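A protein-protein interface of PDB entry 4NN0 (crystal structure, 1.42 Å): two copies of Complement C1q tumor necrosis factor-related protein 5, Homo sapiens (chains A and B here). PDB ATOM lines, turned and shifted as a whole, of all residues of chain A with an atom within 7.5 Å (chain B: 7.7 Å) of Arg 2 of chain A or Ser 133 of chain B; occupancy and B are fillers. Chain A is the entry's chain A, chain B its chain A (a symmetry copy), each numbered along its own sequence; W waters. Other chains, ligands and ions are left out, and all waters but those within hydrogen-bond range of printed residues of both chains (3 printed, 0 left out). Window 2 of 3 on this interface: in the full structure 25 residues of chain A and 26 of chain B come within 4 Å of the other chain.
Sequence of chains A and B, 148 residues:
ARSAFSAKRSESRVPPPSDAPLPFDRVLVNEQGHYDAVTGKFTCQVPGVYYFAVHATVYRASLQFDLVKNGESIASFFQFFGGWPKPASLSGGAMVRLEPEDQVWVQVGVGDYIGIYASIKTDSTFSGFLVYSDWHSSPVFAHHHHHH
OD1 of Asp 134 of chain B lies within salt-bridge range of NH2 of Arg 2 of chain A (3.2 Å). The side-chain hydroxyl (OH) of Tyr 132 of chain B sits at hydrogen-bond distance from the side-chain amide nitrogen (NE2) of Gln 32 of chain A. The side-chain carboxylate of Glu 31 of chain A lies within salt-bridge range of the guanidinium group of Arg 97 of chain B. The side-chain hydroxyl (OH) of Tyr 132 of chain B lies within hydrogen-bond range of the side-chain carboxylate (OE1) of Glu 31 of chain A (2.6 Å). NH1 of Arg 2 of chain A lies within hydrogen-bond range of O of Ser 133 of chain B.
Among the printed residues, pairs that only touch across the chains: Arg 2 of chain A with Tyr 132 of chain B (3.5 Å), Glu 31 of chain A with Val 49 of chain B (3.6 Å), Ala 4 of chain A with Tyr 132 of chain B (3.8 Å) and Phe 129 of chain A with Val 131 of chain B (3.9 Å).
Hydrophobic or aromatic side chains of chain A that line the printed part of chain B: Ala 4 and Phe 129. Hydrophobic or aromatic side chains of chain B that line the printed part of chain A: Val 49, Val 131 and Tyr 132. Along chain B the printed residues that touch a printed residue of chain A span positions 49 to 134.
The side-chain carboxylate (OD2) of Asp 134 of chain B is in hydrogen-bond range of a ring nitrogen (NE2) of His 136 of chain B (3.1 Å). N of Val 49 of chain B lies within hydrogen-bond range of O of Tyr 132 of chain B, 3.0 Å away. The backbone NH of Ala 4 of chain A sits at hydrogen-bond distance from the side-chain amide oxygen of Gln 32 of chain A. N of Val 131 of chain B is in hydrogen-bond range of O of Val 49 of chain B (2.8 Å). NH1 of Arg 97 of chain B is in salt-bridge range of OD2 of Asp 134 of chain B, at 2.9 Å. The backbone NH of Asp 134 of chain B lies within hydrogen-bond range of the backbone carbonyl oxygen of Pro 47 of chain B (2.8 Å).
Ala 1 of chain A touches none of the printed residues of chain B. Arg 2 of chain A touches just these residues of chain B: Tyr 132, Ser 133 and Asp 134. Printed residues of chain B within 4 Å of Gln 32 of chain A: Tyr 132 (3.0 Å). Of the printed residues of chain A, Val 49 of chain B touches Glu 31. Of the printed residues of chain A, Arg 97 of chain B touches Glu 31. Printed residues of chain A within 4 Å of Val 131 of chain B: Phe 129. Ser 133 of chain B touches one residue of chain A. The nearest residue of chain A that does not touch Ser 133 of chain B is Glu 31 of chain A (6.6 Å). The nearest printed residue of chain A that does not touch Arg 97 of chain B is Arg 2 of chain A (6.0 Å).
Water W1 lies within hydrogen-bond range of the backbone carbonyl oxygen of Ala 1 of chain A (2.7 Å) and the backbone carbonyl oxygen of Val 131 of chain B (3.5 Å). Water W2 bridges O of Leu 130 of chain A and O of Val 131 of chain B. Water W3 lies within hydrogen-bond range of O of Ala 4 of chain A (2.8 Å), N of Glu 31 of chain A (2.9 Å) and OH of Tyr 132 of chain B (2.9 Å).
Arg 2 of chain A touches Ser 133 of chain B, but with the chains exchanged Ser 133 of chain A does not touch Arg 2 of chain B (16.0 Å). Positions printed for both chains: 1, 2, 46, 50, 130, 133 and 135. Of the 9 pairs that touch across the chains among the printed residues, none has its exchanged pair printed and touching as well.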
ATOM      1  N   ALA A   1     -22.027  24.059  31.554  1.00  0.00           N
ATOM      2  CA  ALA A   1     -21.479  22.684  31.673  1.00  0.00           C
ATOM      3  C   ALA A   1     -22.259  21.748  30.775  1.00  0.00           C
ATOM      4  O   ALA A   1     -23.387  22.034  30.408  1.00  0.00           O
ATOM      5  CB  ALA A   1     -21.540  22.196  33.101  1.00  0.00           C
ATOM      6  N   ARG A   2     -21.642  20.615  30.458  1.00  0.00           N
ATOM      7  CA  ARG A   2     -22.226  19.627  29.581  1.00  0.00           C
ATOM      8  C   ARG A   2     -21.984  18.229  30.091  1.00  0.00           C
ATOM      9  O   ARG A   2     -20.853  17.886  30.441  1.00  0.00           O
ATOM     10  CB  ARG A   2     -21.574  19.644  28.203  1.00  0.00           C
ATOM     11  CG  ARG A   2     -21.591  20.880  27.466  1.00  0.00           C
ATOM     12  CD  ARG A   2     -20.780  20.610  26.243  1.00  0.00           C
ATOM     13  NE  ARG A   2     -20.660  21.886  25.653  1.00  0.00           N
ATOM     14  CZ  ARG A   2     -20.194  22.121  24.468  1.00  0.00           C
ATOM     15  NH1 ARG A   2     -20.131  23.381  24.070  1.00  0.00           N
ATOM     16  NH2 ARG A   2     -19.813  21.130  23.682  1.00  0.00           N
ATOM     17  N   SER A   3     -23.015  17.406  30.029  1.00  0.00           N
ATOM     18  CA  SER A   3     -22.884  15.999  30.292  1.00  0.00           C
ATOM     19  C   SER A   3     -24.092  15.262  29.731  1.00  0.00           C
ATOM     20  O   SER A   3     -25.243  15.536  30.111  1.00  0.00           O
ATOM     21  CB  SER A   3     -22.779  15.764  31.805  1.00  0.00           C
ATOM     22  OG  SER A   3     -22.637  14.387  32.098  1.00  0.00           O
ATOM     23  N   ALA A   4     -23.844  14.329  28.831  1.00  0.00           N
ATOM     24  CA  ALA A   4     -24.934  13.558  28.236  1.00  0.00           C
ATOM     25  C   ALA A   4     -24.438  12.244  27.702  1.00  0.00           C
ATOM     26  O   ALA A   4     -23.255  12.135  27.263  1.00  0.00           O
ATOM     27  CB  ALA A   4     -25.574  14.324  27.095  1.00  0.00           C
ATOM     28  N   GLU A  31     -19.973  12.150  24.597  1.00  0.00           N
ATOM     29  CA  GLU A  31     -18.876  13.018  24.236  1.00  0.00           C
ATOM     30  C   GLU A  31     -17.936  13.414  25.356  1.00  0.00           C
ATOM     31  O   GLU A  31     -16.799  13.803  25.118  1.00  0.00           O
ATOM     32  CB  GLU A  31     -19.383  14.284  23.533  1.00  0.00           C
ATOM     33  CG  GLU A  31     -20.158  13.994  22.267  1.00  0.00           C
ATOM     34  CD  GLU A  31     -20.649  15.204  21.501  1.00  0.00           C
ATOM     35  OE1 GLU A  31     -20.854  16.290  22.092  1.00  0.00           O
ATOM     36  OE2 GLU A  31     -20.877  15.040  20.272  1.00  0.00           O
ATOM     37  N   GLN A  32     -18.394  13.294  26.590  1.00  0.00           N
ATOM     38  CA  GLN A  32     -17.567  13.567  27.765  1.00  0.00           C
ATOM     39  C   GLN A  32     -16.907  12.330  28.322  1.00  0.00           C
ATOM     40  O   GLN A  32     -16.086  12.423  29.223  1.00  0.00           O
ATOM     41  CB  GLN A  32     -18.405  14.232  28.876  1.00  0.00           C
ATOM     42  CG  GLN A  32     -18.972  15.591  28.503  1.00  0.00           C
ATOM     43  CD  GLN A  32     -20.154  15.522  27.549  1.00  0.00           C
ATOM     44  OE1 GLN A  32     -21.064  14.702  27.713  1.00  0.00           O
ATOM     45  NE2 GLN A  32     -20.133  16.392  26.533  1.00  0.00           N
ATOM     46  N   HIS A  34     -18.484  10.312  30.199  1.00  0.00           N
ATOM     47  CA  HIS A  34     -19.018  10.150  31.542  1.00  0.00           C
ATOM     48  C   HIS A  34     -19.731   8.803  31.712  1.00  0.00           C
ATOM     49  O   HIS A  34     -19.853   8.307  32.837  1.00  0.00           O
ATOM     50  CB  HIS A  34     -19.940  11.308  31.946  1.00  0.00           C
ATOM     51  CG  HIS A  34     -19.238  12.616  32.058  1.00  0.00           C
ATOM     52  ND1 HIS A  34     -19.902  13.815  32.115  1.00  0.00           N
ATOM     53  CD2 HIS A  34     -17.922  12.908  32.184  1.00  0.00           C
ATOM     54  CE1 HIS A  34     -19.037  14.796  32.253  1.00  0.00           C
ATOM     55  NE2 HIS A  34     -17.820  14.274  32.286  1.00  0.00           N
ATOM     56  N   GLN A  45     -19.323  14.006  36.856  1.00  0.00           N
ATOM     57  CA  GLN A  45     -18.199  14.910  37.037  1.00  0.00           C
ATOM     58  C   GLN A  45     -18.635  16.353  37.203  1.00  0.00           C
ATOM     59  O   GLN A  45     -17.812  17.217  37.412  1.00  0.00           O
ATOM     60  CB  GLN A  45     -17.224  14.827  35.869  1.00  0.00           C
ATOM     61  CG  GLN A  45     -16.715  13.431  35.642  1.00  0.00           C
ATOM     62  CD  GLN A  45     -15.859  12.902  36.770  1.00  0.00           C
ATOM     63  OE1 GLN A  45     -15.315  13.654  37.579  1.00  0.00           O
ATOM     64  NE2 GLN A  45     -15.754  11.575  36.842  1.00  0.00           N
ATOM     65  N   VAL A  46     -19.925  16.633  37.057  1.00  0.00           N
ATOM     66  CA  VAL A  46     -20.441  17.964  37.191  1.00  0.00           C
ATOM     67  C   VAL A  46     -21.605  17.906  38.199  1.00  0.00           C
ATOM     68  O   VAL A  46     -22.622  17.238  37.951  1.00  0.00           O
ATOM     69  CB  VAL A  46     -20.983  18.494  35.846  1.00  0.00           C
ATOM     70  CG1 VAL A  46     -21.527  19.901  36.019  1.00  0.00           C
ATOM     71  CG2 VAL A  46     -19.921  18.491  34.768  1.00  0.00           C
ATOM     72  N   TYR A  50     -29.936  15.966  36.970  1.00  0.00           N
ATOM     73  CA  TYR A  50     -29.898  15.152  35.794  1.00  0.00           C
ATOM     74  C   TYR A  50     -31.253  14.482  35.562  1.00  0.00           C
ATOM     75  O   TYR A  50     -31.964  14.144  36.524  1.00  0.00           O
ATOM     76  CB  TYR A  50     -28.855  14.043  35.996  1.00  0.00           C
ATOM     77  CG  TYR A  50     -27.432  14.509  35.997  1.00  0.00           C
ATOM     78  CD1 TYR A  50     -26.882  15.206  37.080  1.00  0.00           C
ATOM     79  CD2 TYR A  50     -26.614  14.288  34.887  1.00  0.00           C
ATOM     80  CE1 TYR A  50     -25.582  15.653  37.047  1.00  0.00           C
ATOM     81  CE2 TYR A  50     -25.312  14.747  34.843  1.00  0.00           C
ATOM     82  CZ  TYR A  50     -24.798  15.430  35.926  1.00  0.00           C
ATOM     83  OH  TYR A  50     -23.504  15.906  35.844  1.00  0.00           O
ATOM     84  N   PHE A 129     -28.717  12.945  31.071  1.00  0.00           N
ATOM     85  CA  PHE A 129     -28.093  14.200  30.790  1.00  0.00           C
ATOM     86  C   PHE A 129     -28.261  15.215  31.920  1.00  0.00           C
ATOM     87  O   PHE A 129     -29.257  15.189  32.660  1.00  0.00           O
ATOM     88  CB  PHE A 129     -28.554  14.832  29.459  1.00  0.00           C
ATOM     89  CG  PHE A 129     -30.069  14.951  29.311  1.00  0.00           C
ATOM     90  CD1 PHE A 129     -30.798  13.907  28.782  1.00  0.00           C
ATOM     91  CD2 PHE A 129     -30.766  16.094  29.724  1.00  0.00           C
ATOM     92  CE1 PHE A 129     -32.166  13.978  28.594  1.00  0.00           C
ATOM     93  CE2 PHE A 129     -32.165  16.168  29.551  1.00  0.00           C
ATOM     94  CZ  PHE A 129     -32.851  15.113  28.989  1.00  0.00           C
ATOM     95  N   LEU A 130     -27.286  16.099  32.056  1.00  0.00           N
ATOM     96  CA  LEU A 130     -27.320  17.249  32.937  1.00  0.00           C
ATOM     97  C   LEU A 130     -28.319  18.267  32.431  1.00  0.00           C
ATOM     98  O   LEU A 130     -28.244  18.663  31.272  1.00  0.00           O
ATOM     99  CB  LEU A 130     -25.932  17.878  32.981  1.00  0.00           C
ATOM    100  CG  LEU A 130     -25.770  19.144  33.805  1.00  0.00           C
ATOM    101  CD1 LEU A 130     -25.639  18.801  35.260  1.00  0.00           C
ATOM    102  CD2 LEU A 130     -24.468  19.816  33.364  1.00  0.00           C
ATOM    103  N   SER A 133     -26.308  22.693  36.072  1.00  0.00           N
ATOM    104  CA  SER A 133     -25.220  22.541  37.002  1.00  0.00           C
ATOM    105  C   SER A 133     -25.482  23.293  38.285  1.00  0.00           C
ATOM    106  O   SER A 133     -26.264  24.254  38.316  1.00  0.00           O
ATOM    107  CB  SER A 133     -23.902  23.012  36.371  1.00  0.00           C
ATOM    108  OG  SER A 133     -23.869  24.395  36.137  1.00  0.00           O
ATOM    109  N   TRP A 135     -22.558  24.154  40.805  1.00  0.00           N
ATOM    110  CA  TRP A 135     -21.271  24.137  41.433  1.00  0.00           C
ATOM    111  C   TRP A 135     -21.257  24.985  42.710  1.00  0.00           C
ATOM    112  O   TRP A 135     -21.962  25.989  42.823  1.00  0.00           O
ATOM    113  CB  TRP A 135     -20.242  24.710  40.491  1.00  0.00           C
ATOM    114  CG  TRP A 135     -19.959  23.932  39.273  1.00  0.00           C
ATOM    115  CD1 TRP A 135     -20.452  24.153  38.013  1.00  0.00           C
ATOM    116  CD2 TRP A 135     -19.017  22.869  39.158  1.00  0.00           C
ATOM    117  NE1 TRP A 135     -19.899  23.267  37.137  1.00  0.00           N
ATOM    118  CE2 TRP A 135     -19.000  22.475  37.805  1.00  0.00           C
ATOM    119  CE3 TRP A 135     -18.201  22.192  40.078  1.00  0.00           C
ATOM    120  CZ2 TRP A 135     -18.197  21.431  37.337  1.00  0.00           C
ATOM    121  CZ3 TRP A 135     -17.372  21.174  39.605  1.00  0.00           C
ATOM    122  CH2 TRP A 135     -17.386  20.802  38.245  1.00  0.00           C
ATOM    123  N   ALA B   1     -27.973  28.528  22.974  1.00  0.00           N
ATOM    124  CA  ALA B   1     -28.803  28.151  21.802  1.00  0.00           C
ATOM    125  C   ALA B   1     -30.068  27.469  22.274  1.00  0.00           C
ATOM    126  O   ALA B   1     -30.123  26.952  23.378  1.00  0.00           O
ATOM    127  CB  ALA B   1     -28.043  27.236  20.870  1.00  0.00           C
ATOM    128  N   ARG B   2     -31.070  27.457  21.401  1.00  0.00           N
ATOM    129  CA  ARG B   2     -32.361  26.882  21.702  1.00  0.00           C
ATOM    130  C   ARG B   2     -32.900  26.101  20.530  1.00  0.00           C
ATOM    131  O   ARG B   2     -32.899  26.599  19.402  1.00  0.00           O
ATOM    132  CB  ARG B   2     -33.411  27.959  21.953  1.00  0.00           C
ATOM    133  CG  ARG B   2     -33.156  28.917  22.997  1.00  0.00           C
ATOM    134  CD  ARG B   2     -34.282  29.893  22.908  1.00  0.00           C
ATOM    135  NE  ARG B   2     -33.894  30.908  23.806  1.00  0.00           N
ATOM    136  CZ  ARG B   2     -34.649  31.881  24.205  1.00  0.00           C
ATOM    137  NH1 ARG B   2     -34.126  32.765  25.040  1.00  0.00           N
ATOM    138  NH2 ARG B   2     -35.905  31.973  23.803  1.00  0.00           N
ATOM    139  N   VAL B  46     -28.757  23.779  14.808  1.00  0.00           N
ATOM    140  CA  VAL B  46     -27.767  24.049  15.810  1.00  0.00           C
ATOM    141  C   VAL B  46     -27.007  22.734  16.069  1.00  0.00           C
ATOM    142  O   VAL B  46     -27.599  21.742  16.524  1.00  0.00           O
ATOM    143  CB  VAL B  46     -28.416  24.508  17.133  1.00  0.00           C
ATOM    144  CG1 VAL B  46     -27.346  24.780  18.175  1.00  0.00           C
ATOM    145  CG2 VAL B  46     -29.266  25.747  16.944  1.00  0.00           C
ATOM    146  N   PRO B  47     -25.690  22.706  15.788  1.00  0.00           N
ATOM    147  CA  PRO B  47     -24.944  21.482  16.119  1.00  0.00           C
ATOM    148  C   PRO B  47     -24.964  21.212  17.626  1.00  0.00           C
ATOM    149  O   PRO B  47     -24.820  22.140  18.449  1.00  0.00           O
ATOM    150  CB  PRO B  47     -23.527  21.791  15.663  1.00  0.00           C
ATOM    151  CG  PRO B  47     -23.420  23.277  15.753  1.00  0.00           C
ATOM    152  CD  PRO B  47     -24.800  23.830  15.469  1.00  0.00           C
ATOM    153  N   GLY B  48     -25.105  19.953  17.994  1.00  0.00           N
ATOM    154  CA  GLY B  48     -25.125  19.623  19.405  1.00  0.00           C
ATOM    155  C   GLY B  48     -25.774  18.289  19.686  1.00  0.00           C
ATOM    156  O   GLY B  48     -26.002  17.489  18.760  1.00  0.00           O
ATOM    157  N   VAL B  49     -26.053  18.033  20.968  1.00  0.00           N
ATOM    158  CA  VAL B  49     -26.614  16.777  21.376  1.00  0.00           C
ATOM    159  C   VAL B  49     -28.054  17.000  21.807  1.00  0.00           C
ATOM    160  O   VAL B  49     -28.348  17.966  22.528  1.00  0.00           O
ATOM    161  CB  VAL B  49     -25.753  16.119  22.469  1.00  0.00           C
ATOM    162  CG1 VAL B  49     -26.416  14.905  23.059  1.00  0.00           C
ATOM    163  CG2 VAL B  49     -24.382  15.734  21.934  1.00  0.00           C
ATOM    164  N   TYR B  50     -28.938  16.133  21.302  1.00  0.00           N
ATOM    165  CA  TYR B  50     -30.361  16.233  21.422  1.00  0.00           C
ATOM    166  C   TYR B  50     -30.931  14.986  22.097  1.00  0.00           C
ATOM    167  O   TYR B  50     -30.404  13.875  21.921  1.00  0.00           O
ATOM    168  CB  TYR B  50     -30.969  16.324  20.014  1.00  0.00           C
ATOM    169  CG  TYR B  50     -30.708  17.612  19.296  1.00  0.00           C
ATOM    170  CD1 TYR B  50     -29.451  17.919  18.759  1.00  0.00           C
ATOM    171  CD2 TYR B  50     -31.717  18.570  19.173  1.00  0.00           C
ATOM    172  CE1 TYR B  50     -29.225  19.122  18.133  1.00  0.00           C
ATOM    173  CE2 TYR B  50     -31.490  19.785  18.557  1.00  0.00           C
ATOM    174  CZ  TYR B  50     -30.242  20.059  18.037  1.00  0.00           C
ATOM    175  OH  TYR B  50     -30.034  21.293  17.454  1.00  0.00           O
ATOM    176  N   ARG B  97     -26.031  13.053  18.490  1.00  0.00           N
ATOM    177  CA  ARG B  97     -25.406  14.269  17.992  1.00  0.00           C
ATOM    178  C   ARG B  97     -25.931  14.584  16.602  1.00  0.00           C
ATOM    179  O   ARG B  97     -26.009  13.688  15.753  1.00  0.00           O
ATOM    180  CB  ARG B  97     -23.879  14.129  17.943  1.00  0.00           C
ATOM    181  CG  ARG B  97     -23.246  15.440  17.534  1.00  0.00           C
ATOM    182  CD  ARG B  97     -21.783  15.468  17.379  1.00  0.00           C
ATOM    183  NE  ARG B  97     -21.383  16.762  16.851  1.00  0.00           N
ATOM    184  CZ  ARG B  97     -20.933  17.748  17.614  1.00  0.00           C
ATOM    185  NH1 ARG B  97     -20.838  17.590  18.927  1.00  0.00           N
ATOM    186  NH2 ARG B  97     -20.529  18.873  17.070  1.00  0.00           N
ATOM    187  N   LEU B 130     -32.643  20.249  22.013  1.00  0.00           N
ATOM    188  CA  LEU B 130     -31.224  20.456  22.217  1.00  0.00           C
ATOM    189  C   LEU B 130     -30.907  20.479  23.697  1.00  0.00           C
ATOM    190  O   LEU B 130     -31.524  21.241  24.435  1.00  0.00           O
ATOM    191  CB  LEU B 130     -30.823  21.786  21.590  1.00  0.00           C
ATOM    192  CG  LEU B 130     -29.377  22.221  21.752  1.00  0.00           C
ATOM    193  CD1 LEU B 130     -28.508  21.512  20.757  1.00  0.00           C
ATOM    194  CD2 LEU B 130     -29.311  23.720  21.449  1.00  0.00           C
ATOM    195  N   VAL B 131     -29.978  19.621  24.104  1.00  0.00           N
ATOM    196  CA  VAL B 131     -29.495  19.568  25.486  1.00  0.00           C
ATOM    197  C   VAL B 131     -28.247  20.446  25.647  1.00  0.00           C
ATOM    198  O   VAL B 131     -28.128  21.177  26.629  1.00  0.00           O
ATOM    199  CB  VAL B 131     -29.256  18.108  25.887  1.00  0.00           C
ATOM    200  CG1 VAL B 131     -28.508  17.997  27.220  1.00  0.00           C
ATOM    201  CG2 VAL B 131     -30.597  17.393  25.961  1.00  0.00           C
ATOM    202  N   TYR B 132     -27.319  20.371  24.700  1.00  0.00           N
ATOM    203  CA  TYR B 132     -26.231  21.336  24.632  1.00  0.00           C
ATOM    204  C   TYR B 132     -25.788  21.534  23.193  1.00  0.00           C
ATOM    205  O   TYR B 132     -25.884  20.626  22.374  1.00  0.00           O
ATOM    206  CB  TYR B 132     -25.055  20.959  25.547  1.00  0.00           C
ATOM    207  CG  TYR B 132     -24.315  19.700  25.217  1.00  0.00           C
ATOM    208  CD1 TYR B 132     -23.431  19.647  24.143  1.00  0.00           C
ATOM    209  CD2 TYR B 132     -24.461  18.549  25.990  1.00  0.00           C
ATOM    210  CE1 TYR B 132     -22.745  18.504  23.867  1.00  0.00           C
ATOM    211  CE2 TYR B 132     -23.755  17.401  25.710  1.00  0.00           C
ATOM    212  CZ  TYR B 132     -22.888  17.394  24.649  1.00  0.00           C
ATOM    213  OH  TYR B 132     -22.155  16.249  24.342  1.00  0.00           O
ATOM    214  N   SER B 133     -25.322  22.734  22.904  1.00  0.00           N
ATOM    215  CA  SER B 133     -24.756  23.052  21.620  1.00  0.00           C
ATOM    216  C   SER B 133     -23.286  22.708  21.566  1.00  0.00           C
ATOM    217  O   SER B 133     -22.608  22.630  22.601  1.00  0.00           O
ATOM    218  CB  SER B 133     -24.965  24.536  21.291  1.00  0.00           C
ATOM    219  OG  SER B 133     -24.236  25.393  22.131  1.00  0.00           O
ATOM    220  N   ASP B 134     -22.794  22.496  20.355  1.00  0.00           N
ATOM    221  CA  ASP B 134     -21.357  22.326  20.157  1.00  0.00           C
ATOM    222  C   ASP B 134     -20.902  22.913  18.844  1.00  0.00           C
ATOM    223  O   ASP B 134     -20.548  22.218  17.902  1.00  0.00           O
ATOM    224  CB  ASP B 134     -20.950  20.875  20.268  1.00  0.00           C
ATOM    225  CG  ASP B 134     -19.435  20.683  20.241  1.00  0.00           C
ATOM    226  OD1 ASP B 134     -18.676  21.550  20.732  1.00  0.00           O
ATOM    227  OD2 ASP B 134     -19.015  19.652  19.706  1.00  0.00           O
ATOM    228  N   TRP B 135     -20.915  24.225  18.788  1.00  0.00           N
ATOM    229  CA  TRP B 135     -20.493  24.889  17.591  1.00  0.00           C
ATOM    230  C   TRP B 135     -18.974  24.801  17.405  1.00  0.00           C
ATOM    231  O   TRP B 135     -18.208  24.768  18.369  1.00  0.00           O
ATOM    232  CB  TRP B 135     -20.861  26.350  17.669  1.00  0.00           C
ATOM    233  CG  TRP B 135     -22.300  26.667  17.663  1.00  0.00           C
ATOM    234  CD1 TRP B 135     -23.089  26.963  18.742  1.00  0.00           C
ATOM    235  CD2 TRP B 135     -23.113  26.844  16.506  1.00  0.00           C
ATOM    236  NE1 TRP B 135     -24.349  27.275  18.326  1.00  0.00           N
ATOM    237  CE2 TRP B 135     -24.393  27.228  16.955  1.00  0.00           C
ATOM    238  CE3 TRP B 135     -22.890  26.689  15.129  1.00  0.00           C
ATOM    239  CZ2 TRP B 135     -25.456  27.464  16.079  1.00  0.00           C
ATOM    240  CZ3 TRP B 135     -23.940  26.960  14.252  1.00  0.00           C
ATOM    241  CH2 TRP B 135     -25.210  27.336  14.737  1.00  0.00           C
ATOM    242  N   HIS B 136     -18.551  24.810  16.150  1.00  0.00           N
ATOM    243  CA  HIS B 136     -17.141  24.931  15.800  1.00  0.00           C
ATOM    244  C   HIS B 136     -16.951  25.890  14.624  1.00  0.00           C
ATOM    245  O   HIS B 136     -17.850  26.046  13.812  1.00  0.00           O
ATOM    246  CB  HIS B 136     -16.615  23.581  15.371  1.00  0.00           C
ATOM    247  CG  HIS B 136     -16.634  22.549  16.447  1.00  0.00           C
ATOM    248  ND1 HIS B 136     -15.884  22.628  17.594  1.00  0.00           N
ATOM    249  CD2 HIS B 136     -17.328  21.400  16.536  1.00  0.00           C
ATOM    250  CE1 HIS B 136     -16.112  21.565  18.344  1.00  0.00           C
ATOM    251  NE2 HIS B 136     -16.988  20.805  17.725  1.00  0.00           N
HETATM  252  O   HOH W   1     -25.728  21.448  29.145  1.00  0.00           O
HETATM  253  O   HOH W   2     -28.972  20.743  29.599  1.00  0.00           O
HETATM  254  O   HOH W   3     -22.565  13.390  24.823  1.00  0.00           O
